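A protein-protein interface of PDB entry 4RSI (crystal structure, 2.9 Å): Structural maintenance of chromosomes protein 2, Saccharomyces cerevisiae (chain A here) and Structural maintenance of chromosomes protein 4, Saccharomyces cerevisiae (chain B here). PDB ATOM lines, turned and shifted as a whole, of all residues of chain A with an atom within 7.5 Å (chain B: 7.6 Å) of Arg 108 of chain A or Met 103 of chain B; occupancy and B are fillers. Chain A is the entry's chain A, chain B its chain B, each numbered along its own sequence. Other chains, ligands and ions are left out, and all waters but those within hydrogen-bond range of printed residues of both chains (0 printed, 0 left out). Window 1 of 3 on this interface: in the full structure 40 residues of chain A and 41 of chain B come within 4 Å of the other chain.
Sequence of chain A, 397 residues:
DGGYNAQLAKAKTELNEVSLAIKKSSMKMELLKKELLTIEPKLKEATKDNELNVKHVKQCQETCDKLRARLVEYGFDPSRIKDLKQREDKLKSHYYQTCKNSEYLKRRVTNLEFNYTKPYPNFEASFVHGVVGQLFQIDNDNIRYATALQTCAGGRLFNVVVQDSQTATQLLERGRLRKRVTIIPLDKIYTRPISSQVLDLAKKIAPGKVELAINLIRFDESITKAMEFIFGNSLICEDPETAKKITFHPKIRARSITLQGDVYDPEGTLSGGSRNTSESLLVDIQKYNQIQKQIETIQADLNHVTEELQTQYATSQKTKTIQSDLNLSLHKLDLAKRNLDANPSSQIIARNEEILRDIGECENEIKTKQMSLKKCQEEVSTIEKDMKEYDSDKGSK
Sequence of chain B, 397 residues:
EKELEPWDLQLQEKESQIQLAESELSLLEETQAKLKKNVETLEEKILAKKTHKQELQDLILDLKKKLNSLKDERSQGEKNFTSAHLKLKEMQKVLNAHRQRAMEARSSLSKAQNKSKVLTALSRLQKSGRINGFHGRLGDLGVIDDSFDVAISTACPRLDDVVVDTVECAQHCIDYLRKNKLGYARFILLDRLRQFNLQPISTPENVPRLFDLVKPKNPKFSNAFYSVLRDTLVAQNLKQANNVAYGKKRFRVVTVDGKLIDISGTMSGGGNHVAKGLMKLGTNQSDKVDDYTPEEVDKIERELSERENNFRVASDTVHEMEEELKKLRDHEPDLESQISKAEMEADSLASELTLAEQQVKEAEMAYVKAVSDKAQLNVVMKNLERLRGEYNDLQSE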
ATOM      1  N   SER A 102      22.787   6.821   5.302  1.00  0.00           N
ATOM      2  CA  SER A 102      23.307   5.759   6.170  1.00  0.00           C
ATOM      3  C   SER A 102      23.640   4.497   5.417  1.00  0.00           C
ATOM      4  O   SER A 102      24.452   3.708   5.866  1.00  0.00           O
ATOM      5  CB  SER A 102      22.305   5.412   7.262  1.00  0.00           C
ATOM      6  OG  SER A 102      21.972   6.577   7.973  1.00  0.00           O
ATOM      7  N   GLU A 103      22.995   4.310   4.275  1.00  0.00           N
ATOM      8  CA  GLU A 103      23.193   3.128   3.454  1.00  0.00           C
ATOM      9  C   GLU A 103      24.679   2.832   3.214  1.00  0.00           C
ATOM     10  O   GLU A 103      25.071   1.665   3.133  1.00  0.00           O
ATOM     11  CB  GLU A 103      22.451   3.279   2.118  1.00  0.00           C
ATOM     12  CG  GLU A 103      21.929   1.971   1.527  1.00  0.00           C
ATOM     13  CD  GLU A 103      20.673   1.465   2.237  1.00  0.00           C
ATOM     14  OE1 GLU A 103      20.102   2.252   3.031  1.00  0.00           O
ATOM     15  OE2 GLU A 103      20.256   0.294   1.998  1.00  0.00           O
ATOM     16  N   TYR A 104      25.506   3.874   3.125  1.00  0.00           N
ATOM     17  CA  TYR A 104      26.930   3.651   2.897  1.00  0.00           C
ATOM     18  C   TYR A 104      27.459   2.787   4.028  1.00  0.00           C
ATOM     19  O   TYR A 104      28.253   1.870   3.814  1.00  0.00           O
ATOM     20  CB  TYR A 104      27.709   4.972   2.816  1.00  0.00           C
ATOM     21  CG  TYR A 104      28.186   5.507   4.156  1.00  0.00           C
ATOM     22  CD1 TYR A 104      27.321   6.192   5.001  1.00  0.00           C
ATOM     23  CD2 TYR A 104      29.498   5.322   4.582  1.00  0.00           C
ATOM     24  CE1 TYR A 104      27.743   6.683   6.240  1.00  0.00           C
ATOM     25  CE2 TYR A 104      29.932   5.805   5.825  1.00  0.00           C
ATOM     26  CZ  TYR A 104      29.047   6.486   6.650  1.00  0.00           C
ATOM     27  OH  TYR A 104      29.454   6.977   7.880  1.00  0.00           O
ATOM     28  N   LEU A 105      26.964   3.072   5.227  1.00  0.00           N
ATOM     29  CA  LEU A 105      27.471   2.485   6.452  1.00  0.00           C
ATOM     30  C   LEU A 105      26.971   1.048   6.592  1.00  0.00           C
ATOM     31  O   LEU A 105      27.735   0.155   6.925  1.00  0.00           O
ATOM     32  CB  LEU A 105      27.062   3.361   7.640  1.00  0.00           C
ATOM     33  CG  LEU A 105      27.512   2.945   9.036  1.00  0.00           C
ATOM     34  CD1 LEU A 105      29.021   2.730   9.040  1.00  0.00           C
ATOM     35  CD2 LEU A 105      27.106   3.982  10.083  1.00  0.00           C
ATOM     36  N   LYS A 106      25.697   0.835   6.281  1.00  0.00           N
ATOM     37  CA  LYS A 106      25.066  -0.490   6.257  1.00  0.00           C
ATOM     38  C   LYS A 106      25.822  -1.533   5.429  1.00  0.00           C
ATOM     39  O   LYS A 106      25.656  -2.727   5.634  1.00  0.00           O
ATOM     40  CB  LYS A 106      23.635  -0.368   5.704  1.00  0.00           C
ATOM     41  CG  LYS A 106      22.637  -1.435   6.169  1.00  0.00           C
ATOM     42  CD  LYS A 106      21.302  -1.279   5.416  1.00  0.00           C
ATOM     43  CE  LYS A 106      20.112  -1.803   6.215  1.00  0.00           C
ATOM     44  NZ  LYS A 106      19.871  -0.939   7.402  1.00  0.00           N
ATOM     45  N   ARG A 107      26.642  -1.090   4.489  1.00  0.00           N
ATOM     46  CA  ARG A 107      27.381  -2.037   3.653  1.00  0.00           C
ATOM     47  C   ARG A 107      28.523  -2.721   4.415  1.00  0.00           C
ATOM     48  O   ARG A 107      28.820  -3.890   4.169  1.00  0.00           O
ATOM     49  CB  ARG A 107      27.917  -1.354   2.381  1.00  0.00           C
ATOM     50  CG  ARG A 107      26.915  -0.392   1.693  1.00  0.00           C
ATOM     51  CD  ARG A 107      27.434   0.160   0.356  1.00  0.00           C
ATOM     52  NE  ARG A 107      26.658   1.316  -0.111  1.00  0.00           N
ATOM     53  CZ  ARG A 107      26.985   2.090  -1.147  1.00  0.00           C
ATOM     54  NH1 ARG A 107      28.083   1.835  -1.857  1.00  0.00           N
ATOM     55  NH2 ARG A 107      26.210   3.127  -1.475  1.00  0.00           N
ATOM     56  N   ARG A 108      29.148  -1.993   5.340  1.00  0.00           N
ATOM     57  CA  ARG A 108      30.306  -2.507   6.057  1.00  0.00           C
ATOM     58  C   ARG A 108      29.937  -3.245   7.336  1.00  0.00           C
ATOM     59  O   ARG A 108      30.773  -3.866   7.964  1.00  0.00           O
ATOM     60  CB  ARG A 108      31.278  -1.372   6.385  1.00  0.00           C
ATOM     61  CG  ARG A 108      32.035  -0.812   5.170  1.00  0.00           C
ATOM     62  CD  ARG A 108      33.362  -0.104   5.544  1.00  0.00           C
ATOM     63  NE  ARG A 108      33.192   1.048   6.436  1.00  0.00           N
ATOM     64  CZ  ARG A 108      32.647   2.211   6.076  1.00  0.00           C
ATOM     65  NH1 ARG A 108      32.194   2.390   4.837  1.00  0.00           N
ATOM     66  NH2 ARG A 108      32.552   3.193   6.965  1.00  0.00           N
ATOM     67  N   VAL A 109      28.676  -3.164   7.722  1.00  0.00           N
ATOM     68  CA  VAL A 109      28.216  -3.727   8.981  1.00  0.00           C
ATOM     69  C   VAL A 109      27.181  -4.813   8.676  1.00  0.00           C
ATOM     70  O   VAL A 109      25.986  -4.640   8.905  1.00  0.00           O
ATOM     71  CB  VAL A 109      27.647  -2.596   9.863  1.00  0.00           C
ATOM     72  CG1 VAL A 109      27.060  -3.120  11.144  1.00  0.00           C
ATOM     73  CG2 VAL A 109      28.754  -1.637  10.202  1.00  0.00           C
ATOM     74  N   THR A 110      27.640  -5.931   8.127  1.00  0.00           N
ATOM     75  CA  THR A 110      26.713  -6.875   7.507  1.00  0.00           C
ATOM     76  C   THR A 110      26.341  -7.979   8.471  1.00  0.00           C
ATOM     77  O   THR A 110      25.176  -8.352   8.597  1.00  0.00           O
ATOM     78  CB  THR A 110      27.303  -7.487   6.224  1.00  0.00           C
ATOM     79  OG1 THR A 110      28.134  -6.517   5.584  1.00  0.00           O
ATOM     80  CG2 THR A 110      26.213  -7.897   5.262  1.00  0.00           C
ATOM     81  N   ASN A 111      27.341  -8.498   9.155  1.00  0.00           N
ATOM     82  CA  ASN A 111      27.134  -9.544  10.128  1.00  0.00           C
ATOM     83  C   ASN A 111      26.328  -9.108  11.349  1.00  0.00           C
ATOM     84  O   ASN A 111      26.161  -9.869  12.288  1.00  0.00           O
ATOM     85  CB  ASN A 111      28.487 -10.085  10.590  1.00  0.00           C
ATOM     86  CG  ASN A 111      29.439 -10.369   9.435  1.00  0.00           C
ATOM     87  OD1 ASN A 111      29.198 -11.266   8.619  1.00  0.00           O
ATOM     88  ND2 ASN A 111      30.544  -9.616   9.374  1.00  0.00           N
ATOM     89  N   LEU A 112      25.815  -7.893  11.365  1.00  0.00           N
ATOM     90  CA  LEU A 112      25.012  -7.499  12.506  1.00  0.00           C
ATOM     91  C   LEU A 112      23.585  -8.036  12.388  1.00  0.00           C
ATOM     92  O   LEU A 112      22.775  -7.887  13.307  1.00  0.00           O
ATOM     93  CB  LEU A 112      24.994  -5.983  12.638  1.00  0.00           C
ATOM     94  CG  LEU A 112      25.938  -5.355  13.649  1.00  0.00           C
ATOM     95  CD1 LEU A 112      25.396  -4.005  14.009  1.00  0.00           C
ATOM     96  CD2 LEU A 112      26.077  -6.197  14.890  1.00  0.00           C
ATOM     97  N   PHE A 158      29.312 -11.241  16.865  1.00  0.00           N
ATOM     98  CA  PHE A 158      28.177 -11.640  16.027  1.00  0.00           C
ATOM     99  C   PHE A 158      27.400 -12.857  16.556  1.00  0.00           C
ATOM    100  O   PHE A 158      26.536 -13.406  15.897  1.00  0.00           O
ATOM    101  CB  PHE A 158      28.677 -11.857  14.610  1.00  0.00           C
ATOM    102  CG  PHE A 158      29.449 -10.686  14.082  1.00  0.00           C
ATOM    103  CD1 PHE A 158      29.177  -9.400  14.534  1.00  0.00           C
ATOM    104  CD2 PHE A 158      30.441 -10.855  13.133  1.00  0.00           C
ATOM    105  CE1 PHE A 158      29.873  -8.325  14.059  1.00  0.00           C
ATOM    106  CE2 PHE A 158      31.139  -9.760  12.639  1.00  0.00           C
ATOM    107  CZ  PHE A 158      30.853  -8.500  13.108  1.00  0.00           C
ATOM    108  N   SER A 280      38.066   0.506  12.966  1.00  0.00           N
ATOM    109  CA  SER A 280      37.667  -0.611  12.114  1.00  0.00           C
ATOM    110  C   SER A 280      36.170  -0.923  12.262  1.00  0.00           C
ATOM    111  O   SER A 280      35.310  -0.031  12.154  1.00  0.00           O
ATOM    112  CB  SER A 280      38.512  -1.843  12.427  1.00  0.00           C
ATOM    113  N   LEU A 281      35.876  -2.193  12.526  1.00  0.00           N
ATOM    114  CA  LEU A 281      34.508  -2.686  12.590  1.00  0.00           C
ATOM    115  C   LEU A 281      33.732  -2.148  13.786  1.00  0.00           C
ATOM    116  O   LEU A 281      32.702  -1.512  13.623  1.00  0.00           O
ATOM    117  CB  LEU A 281      34.513  -4.211  12.649  1.00  0.00           C
ATOM    118  CG  LEU A 281      33.572  -4.950  11.719  1.00  0.00           C
ATOM    119  CD1 LEU A 281      33.810  -6.410  11.882  1.00  0.00           C
ATOM    120  CD2 LEU A 281      32.157  -4.635  12.052  1.00  0.00           C
ATOM    121  N   ASP A 284      32.130   1.352  13.297  1.00  0.00           N
ATOM    122  CA  ASP A 284      31.037   1.519  12.347  1.00  0.00           C
ATOM    123  C   ASP A 284      29.774   0.906  12.942  1.00  0.00           C
ATOM    124  O   ASP A 284      28.679   1.420  12.766  1.00  0.00           O
ATOM    125  CB  ASP A 284      31.376   0.869  11.001  1.00  0.00           C
ATOM    126  CG  ASP A 284      32.550   1.539  10.302  1.00  0.00           C
ATOM    127  OD1 ASP A 284      32.754   2.749  10.539  1.00  0.00           O
ATOM    128  OD2 ASP A 284      33.265   0.868   9.514  1.00  0.00           O
ATOM    129  N   ILE A 285      29.944  -0.191  13.666  1.00  0.00           N
ATOM    130  CA  ILE A 285      28.842  -0.845  14.346  1.00  0.00           C
ATOM    131  C   ILE A 285      28.169   0.119  15.319  1.00  0.00           C
ATOM    132  O   ILE A 285      26.948   0.283  15.300  1.00  0.00           O
ATOM    133  CB  ILE A 285      29.329  -2.078  15.114  1.00  0.00           C
ATOM    134  CG1 ILE A 285      29.722  -3.181  14.142  1.00  0.00           C
ATOM    135  CG2 ILE A 285      28.244  -2.610  16.012  1.00  0.00           C
ATOM    136  CD1 ILE A 285      30.338  -4.329  14.841  1.00  0.00           C
ATOM    137  N   TYR A 288      26.418   2.743  13.323  1.00  0.00           N
ATOM    138  CA  TYR A 288      25.225   2.172  12.746  1.00  0.00           C
ATOM    139  C   TYR A 288      24.135   2.029  13.806  1.00  0.00           C
ATOM    140  O   TYR A 288      22.994   2.398  13.567  1.00  0.00           O
ATOM    141  CB  TYR A 288      25.576   0.843  12.098  1.00  0.00           C
ATOM    142  CG  TYR A 288      24.411   0.075  11.564  1.00  0.00           C
ATOM    143  CD1 TYR A 288      23.694  -0.765  12.387  1.00  0.00           C
ATOM    144  CD2 TYR A 288      24.043   0.152  10.227  1.00  0.00           C
ATOM    145  CE1 TYR A 288      22.625  -1.500  11.914  1.00  0.00           C
ATOM    146  CE2 TYR A 288      22.956  -0.597   9.738  1.00  0.00           C
ATOM    147  CZ  TYR A 288      22.259  -1.418  10.599  1.00  0.00           C
ATOM    148  OH  TYR A 288      21.194  -2.171  10.178  1.00  0.00           O
ATOM    149  N   ALA B  97      20.781  -9.906   0.391  1.00  0.00           N
ATOM    150  CA  ALA B  97      21.349 -11.205   0.042  1.00  0.00           C
ATOM    151  C   ALA B  97      22.767 -11.101  -0.524  1.00  0.00           C
ATOM    152  O   ALA B  97      23.694 -11.711   0.001  1.00  0.00           O
ATOM    153  CB  ALA B  97      20.465 -11.907  -0.949  1.00  0.00           C
ATOM    154  N   HIS B  98      22.941 -10.331  -1.591  1.00  0.00           N
ATOM    155  CA  HIS B  98      24.249 -10.235  -2.234  1.00  0.00           C
ATOM    156  C   HIS B  98      25.289  -9.552  -1.348  1.00  0.00           C
ATOM    157  O   HIS B  98      26.472  -9.870  -1.419  1.00  0.00           O
ATOM    158  CB  HIS B  98      24.148  -9.553  -3.602  1.00  0.00           C
ATOM    159  CG  HIS B  98      23.363 -10.341  -4.614  1.00  0.00           C
ATOM    160  ND1 HIS B  98      23.699 -10.374  -5.947  1.00  0.00           N
ATOM    161  CD2 HIS B  98      22.258 -11.113  -4.475  1.00  0.00           C
ATOM    162  CE1 HIS B  98      22.835 -11.147  -6.593  1.00  0.00           C
ATOM    163  NE2 HIS B  98      21.953 -11.602  -5.730  1.00  0.00           N
ATOM    164  N   ARG B  99      24.844  -8.619  -0.513  1.00  0.00           N
ATOM    165  CA  ARG B  99      25.729  -7.974   0.441  1.00  0.00           C
ATOM    166  C   ARG B  99      26.329  -9.007   1.392  1.00  0.00           C
ATOM    167  O   ARG B  99      27.507  -8.948   1.716  1.00  0.00           O
ATOM    168  CB  ARG B  99      24.963  -6.935   1.255  1.00  0.00           C
ATOM    169  CG  ARG B  99      24.929  -5.546   0.666  1.00  0.00           C
ATOM    170  CD  ARG B  99      24.312  -4.536   1.632  1.00  0.00           C
ATOM    171  NE  ARG B  99      23.873  -3.337   0.923  1.00  0.00           N
ATOM    172  CZ  ARG B  99      23.046  -2.436   1.430  1.00  0.00           C
ATOM    173  NH1 ARG B  99      22.685  -1.376   0.722  1.00  0.00           N
ATOM    174  NH2 ARG B  99      22.583  -2.604   2.652  1.00  0.00           N
ATOM    175  N   GLN B 100      25.503  -9.944   1.853  1.00  0.00           N
ATOM    176  CA  GLN B 100      25.958 -11.004   2.755  1.00  0.00           C
ATOM    177  C   GLN B 100      27.030 -11.851   2.104  1.00  0.00           C
ATOM    178  O   GLN B 100      28.148 -11.943   2.607  1.00  0.00           O
ATOM    179  CB  GLN B 100      24.791 -11.894   3.175  1.00  0.00           C
ATOM    180  CG  GLN B 100      23.840 -11.231   4.145  1.00  0.00           C
ATOM    181  CD  GLN B 100      24.399 -11.157   5.542  1.00  0.00           C
ATOM    182  OE1 GLN B 100      25.505 -11.651   5.818  1.00  0.00           O
ATOM    183  NE2 GLN B 100      23.637 -10.542   6.448  1.00  0.00           N
ATOM    184  N   ARG B 101      26.670 -12.464   0.982  1.00  0.00           N
ATOM    185  CA  ARG B 101      27.601 -13.250   0.190  1.00  0.00           C
ATOM    186  C   ARG B 101      28.886 -12.484  -0.136  1.00  0.00           C
ATOM    187  O   ARG B 101      29.974 -13.026   0.000  1.00  0.00           O
ATOM    188  CB  ARG B 101      26.919 -13.772  -1.078  1.00  0.00           C
ATOM    189  CG  ARG B 101      25.756 -14.740  -0.786  1.00  0.00           C
ATOM    190  CD  ARG B 101      25.314 -15.523  -2.042  1.00  0.00           C
ATOM    191  NE  ARG B 101      24.116 -14.974  -2.688  1.00  0.00           N
ATOM    192  CZ  ARG B 101      23.926 -14.905  -4.007  1.00  0.00           C
ATOM    193  NH1 ARG B 101      24.851 -15.350  -4.853  1.00  0.00           N
ATOM    194  NH2 ARG B 101      22.805 -14.380  -4.481  1.00  0.00           N
ATOM    195  N   ALA B 102      28.777 -11.225  -0.536  1.00  0.00           N
ATOM    196  CA  ALA B 102      29.983 -10.444  -0.800  1.00  0.00           C
ATOM    197  C   ALA B 102      30.934 -10.419   0.409  1.00  0.00           C
ATOM    198  O   ALA B 102      32.088 -10.772   0.269  1.00  0.00           O
ATOM    199  CB  ALA B 102      29.639  -9.045  -1.252  1.00  0.00           C
ATOM    200  N   MET B 103      30.455 -10.036   1.588  1.00  0.00           N
ATOM    201  CA  MET B 103      31.287 -10.079   2.796  1.00  0.00           C
ATOM    202  C   MET B 103      31.903 -11.465   3.090  1.00  0.00           C
ATOM    203  O   MET B 103      33.075 -11.551   3.466  1.00  0.00           O
ATOM    204  CB  MET B 103      30.517  -9.573   4.029  1.00  0.00           C
ATOM    205  CG  MET B 103      31.260  -9.742   5.375  1.00  0.00           C
ATOM    206  SD  MET B 103      32.531  -8.490   5.735  1.00  0.00           S
ATOM    207  CE  MET B 103      31.505  -7.066   6.165  1.00  0.00           C
ATOM    208  N   GLU B 104      31.127 -12.534   2.923  1.00  0.00           N
ATOM    209  CA  GLU B 104      31.644 -13.876   3.150  1.00  0.00           C
ATOM    210  C   GLU B 104      32.807 -14.154   2.220  1.00  0.00           C
ATOM    211  O   GLU B 104      33.905 -14.491   2.653  1.00  0.00           O
ATOM    212  CB  GLU B 104      30.549 -14.924   2.931  1.00  0.00           C
ATOM    213  CG  GLU B 104      29.346 -14.737   3.845  1.00  0.00           C
ATOM    214  CD  GLU B 104      28.184 -15.681   3.528  1.00  0.00           C
ATOM    215  OE1 GLU B 104      28.448 -16.812   3.048  1.00  0.00           O
ATOM    216  OE2 GLU B 104      27.011 -15.279   3.769  1.00  0.00           O
ATOM    217  N   ALA B 105      32.539 -14.007   0.932  1.00  0.00           N
ATOM    218  CA  ALA B 105      33.518 -14.295  -0.090  1.00  0.00           C
ATOM    219  C   ALA B 105      34.767 -13.461   0.117  1.00  0.00           C
ATOM    220  O   ALA B 105      35.872 -13.937  -0.098  1.00  0.00           O
ATOM    221  CB  ALA B 105      32.930 -14.045  -1.463  1.00  0.00           C
ATOM    222  N   ARG B 106      34.596 -12.216   0.541  1.00  0.00           N
ATOM    223  CA  ARG B 106      35.740 -11.350   0.766  1.00  0.00           C
ATOM    224  C   ARG B 106      36.443 -11.769   2.036  1.00  0.00           C
ATOM    225  O   ARG B 106      37.661 -11.897   2.049  1.00  0.00           O
ATOM    226  CB  ARG B 106      35.334  -9.869   0.824  1.00  0.00           C
ATOM    227  CG  ARG B 106      36.465  -8.902   1.212  1.00  0.00           C
ATOM    228  CD  ARG B 106      37.748  -9.133   0.413  1.00  0.00           C
ATOM    229  NE  ARG B 106      37.608  -8.819  -1.014  1.00  0.00           N
ATOM    230  CZ  ARG B 106      38.614  -8.836  -1.887  1.00  0.00           C
ATOM    231  NH1 ARG B 106      39.844  -9.146  -1.485  1.00  0.00           N
ATOM    232  NH2 ARG B 106      38.393  -8.539  -3.163  1.00  0.00           N
ATOM    233  N   SER B 107      35.672 -11.991   3.096  1.00  0.00           N
ATOM    234  CA  SER B 107      36.237 -12.388   4.380  1.00  0.00           C
ATOM    235  C   SER B 107      37.103 -13.609   4.240  1.00  0.00           C
ATOM    236  O   SER B 107      38.222 -13.632   4.734  1.00  0.00           O
ATOM    237  CB  SER B 107      35.146 -12.682   5.404  1.00  0.00           C
ATOM    238  OG  SER B 107      35.087 -11.668   6.386  1.00  0.00           O
ATOM    239  N   SER B 108      36.585 -14.624   3.561  1.00  0.00           N
ATOM    240  CA  SER B 108      37.294 -15.890   3.473  1.00  0.00           C
ATOM    241  C   SER B 108      38.556 -15.797   2.602  1.00  0.00           C
ATOM    242  O   SER B 108      39.577 -16.385   2.930  1.00  0.00           O
ATOM    243  CB  SER B 108      36.362 -16.995   3.000  1.00  0.00           C
ATOM    244  OG  SER B 108      36.072 -16.843   1.624  1.00  0.00           O
ATOM    245  N   LEU B 109      38.501 -15.043   1.512  1.00  0.00           N
ATOM    246  CA  LEU B 109      39.675 -14.885   0.650  1.00  0.00           C
ATOM    247  C   LEU B 109      40.750 -14.057   1.351  1.00  0.00           C
ATOM    248  O   LEU B 109      41.916 -14.037   0.947  1.00  0.00           O
ATOM    249  CB  LEU B 109      39.291 -14.217  -0.671  1.00  0.00           C
ATOM    250  CG  LEU B 109      40.392 -14.111  -1.724  1.00  0.00           C
ATOM    251  CD1 LEU B 109      40.923 -15.495  -2.045  1.00  0.00           C
ATOM    252  CD2 LEU B 109      39.865 -13.434  -2.968  1.00  0.00           C
ATOM    253  N   SER B 110      40.344 -13.360   2.401  1.00  0.00           N
ATOM    254  CA  SER B 110      41.271 -12.555   3.147  1.00  0.00           C
ATOM    255  C   SER B 110      41.905 -13.457   4.166  1.00  0.00           C
ATOM    256  O   SER B 110      43.078 -13.296   4.493  1.00  0.00           O
ATOM    257  CB  SER B 110      40.553 -11.396   3.839  1.00  0.00           C
ATOM    258  OG  SER B 110      40.041 -10.452   2.901  1.00  0.00           O
ATOM    259  N   ILE B 300      32.443 -10.645  -7.878  1.00  0.00           N
ATOM    260  CA  ILE B 300      31.280 -10.515  -7.014  1.00  0.00           C
ATOM    261  C   ILE B 300      31.240  -9.121  -6.377  1.00  0.00           C
ATOM    262  O   ILE B 300      30.181  -8.499  -6.266  1.00  0.00           O
ATOM    263  CB  ILE B 300      31.254 -11.629  -5.966  1.00  0.00           C
ATOM    264  CG1 ILE B 300      31.009 -12.967  -6.661  1.00  0.00           C
ATOM    265  CG2 ILE B 300      30.179 -11.380  -4.925  1.00  0.00           C
ATOM    266  CD1 ILE B 300      30.896 -14.132  -5.714  1.00  0.00           C
ATOM    267  N   GLU B 301      32.402  -8.613  -5.993  1.00  0.00           N
ATOM    268  CA  GLU B 301      32.478  -7.258  -5.478  1.00  0.00           C
ATOM    269  C   GLU B 301      32.278  -6.242  -6.606  1.00  0.00           C
ATOM    270  O   GLU B 301      32.154  -5.043  -6.357  1.00  0.00           O
ATOM    271  CB  GLU B 301      33.802  -7.035  -4.733  1.00  0.00           C
ATOM    272  CG  GLU B 301      33.844  -7.666  -3.341  1.00  0.00           C
ATOM    273  CD  GLU B 301      35.023  -7.193  -2.482  1.00  0.00           C
ATOM    274  OE1 GLU B 301      36.144  -7.064  -3.020  1.00  0.00           O
ATOM    275  OE2 GLU B 301      34.831  -6.956  -1.263  1.00  0.00           O
ATOM    276  N   LEU B 304      28.039  -6.381  -7.193  1.00  0.00           N
ATOM    277  CA  LEU B 304      27.340  -5.809  -6.048  1.00  0.00           C
ATOM    278  C   LEU B 304      27.245  -4.305  -6.223  1.00  0.00           C
ATOM    279  O   LEU B 304      26.209  -3.708  -5.933  1.00  0.00           O
ATOM    280  CB  LEU B 304      28.029  -6.129  -4.724  1.00  0.00           C
ATOM    281  CG  LEU B 304      27.451  -5.382  -3.508  1.00  0.00           C
ATOM    282  CD1 LEU B 304      26.297  -6.134  -2.871  1.00  0.00           C
ATOM    283  CD2 LEU B 304      28.519  -5.074  -2.468  1.00  0.00           C
ATOM    284  N   GLU B 308      23.995  -2.420  -6.125  1.00  0.00           N
ATOM    285  CA  GLU B 308      23.923  -1.392  -5.077  1.00  0.00           C
ATOM    286  C   GLU B 308      23.386  -0.082  -5.628  1.00  0.00           C
ATOM    287  O   GLU B 308      22.613   0.615  -4.965  1.00  0.00           O
ATOM    288  CB  GLU B 308      25.290  -1.139  -4.428  1.00  0.00           C
ATOM    289  CG  GLU B 308      25.596  -2.006  -3.207  1.00  0.00           C
ATOM    290  CD  GLU B 308      25.162  -1.360  -1.897  1.00  0.00           C
ATOM    291  OE1 GLU B 308      25.482  -1.929  -0.822  1.00  0.00           O
ATOM    292  OE2 GLU B 308      24.503  -0.290  -1.950  1.00  0.00           O
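Arg 99 of chain B touches Lys 106 of chain A. CE of Met 103 of chain B touches O of Arg 108 of chain A, 3.7 Å away. Arg 99 of chain B touches Thr 110 of chain A (O to CG2, 3.9 Å). Thr 110 of chain A touches Met 103 of chain B.
Of the printed residues of chain B, Glu 103 of chain A touches Arg 99. Printed residues of chain B within 4 Å of Arg 107 of chain A: Glu 308 (3.1 Å). Of chain B, only Met 103 comes within 4 Å of Arg 108 of chain A. Of the printed residues of chain B, Thr 110 of chain A touches Arg 99 (3.9 Å), Gln 100 (3.4 Å) and Met 103 (3.5 Å). Asn 111 of chain A touches none of the printed residues of chain B. No residue of chain A comes within 4 Å of Ala 102 of chain B. Printed residues of chain A within 4 Å of Glu 308 of chain B: Arg 107 (3.1 Å).
OE2 of Glu 308 of chain B lies within salt-bridge range of NE of Arg 107 of chain A, at 3.3 Å. NE2 of Gln 100 of chain B is in hydrogen-bond range of O of Thr 110 of chain A, at 3.4 Å. The guanidinium group of Arg 99 of chain B lies within salt-bridge range of the side-chain carboxylate of Glu 103 of chain A.
Of the 18 printed residues of chain B, 4 touch a printed residue of chain A. Printed residues of chain B that touch a printed residue of chain A: Arg 99, Gln 100, Met 103 and Glu 308. Hydrophobic or aromatic side chains of chain B that line the printed part of chain A: Met 103. Of the 17 printed residues of chain A, 5 touch a printed residue of chain B. Among the printed residues, 7 pairs touch across the chains.
The side-chain carboxylate (OE1) of Glu 308 of chain B is in salt-bridge range of the guanidinium group (NE) of Arg 99 of chain B (2.8 Å). The side-chain carboxylate (OD2) of Asp 284 of chain A is in salt-bridge range of the guanidinium group (NE) of Arg 108 of chain A, at 3.1 Å. The backbone carbonyl oxygen (O) of Arg 107 of chain A lies within hydrogen-bond range of the side-chain hydroxyl (OG1) of Thr 110 of chain A, 3.1 Å away. The side-chain amino group (NZ) of Lys 106 of chain A lies within hydrogen-bond range of the side-chain hydroxyl (OH) of Tyr 288 of chain A (3.3 Å).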
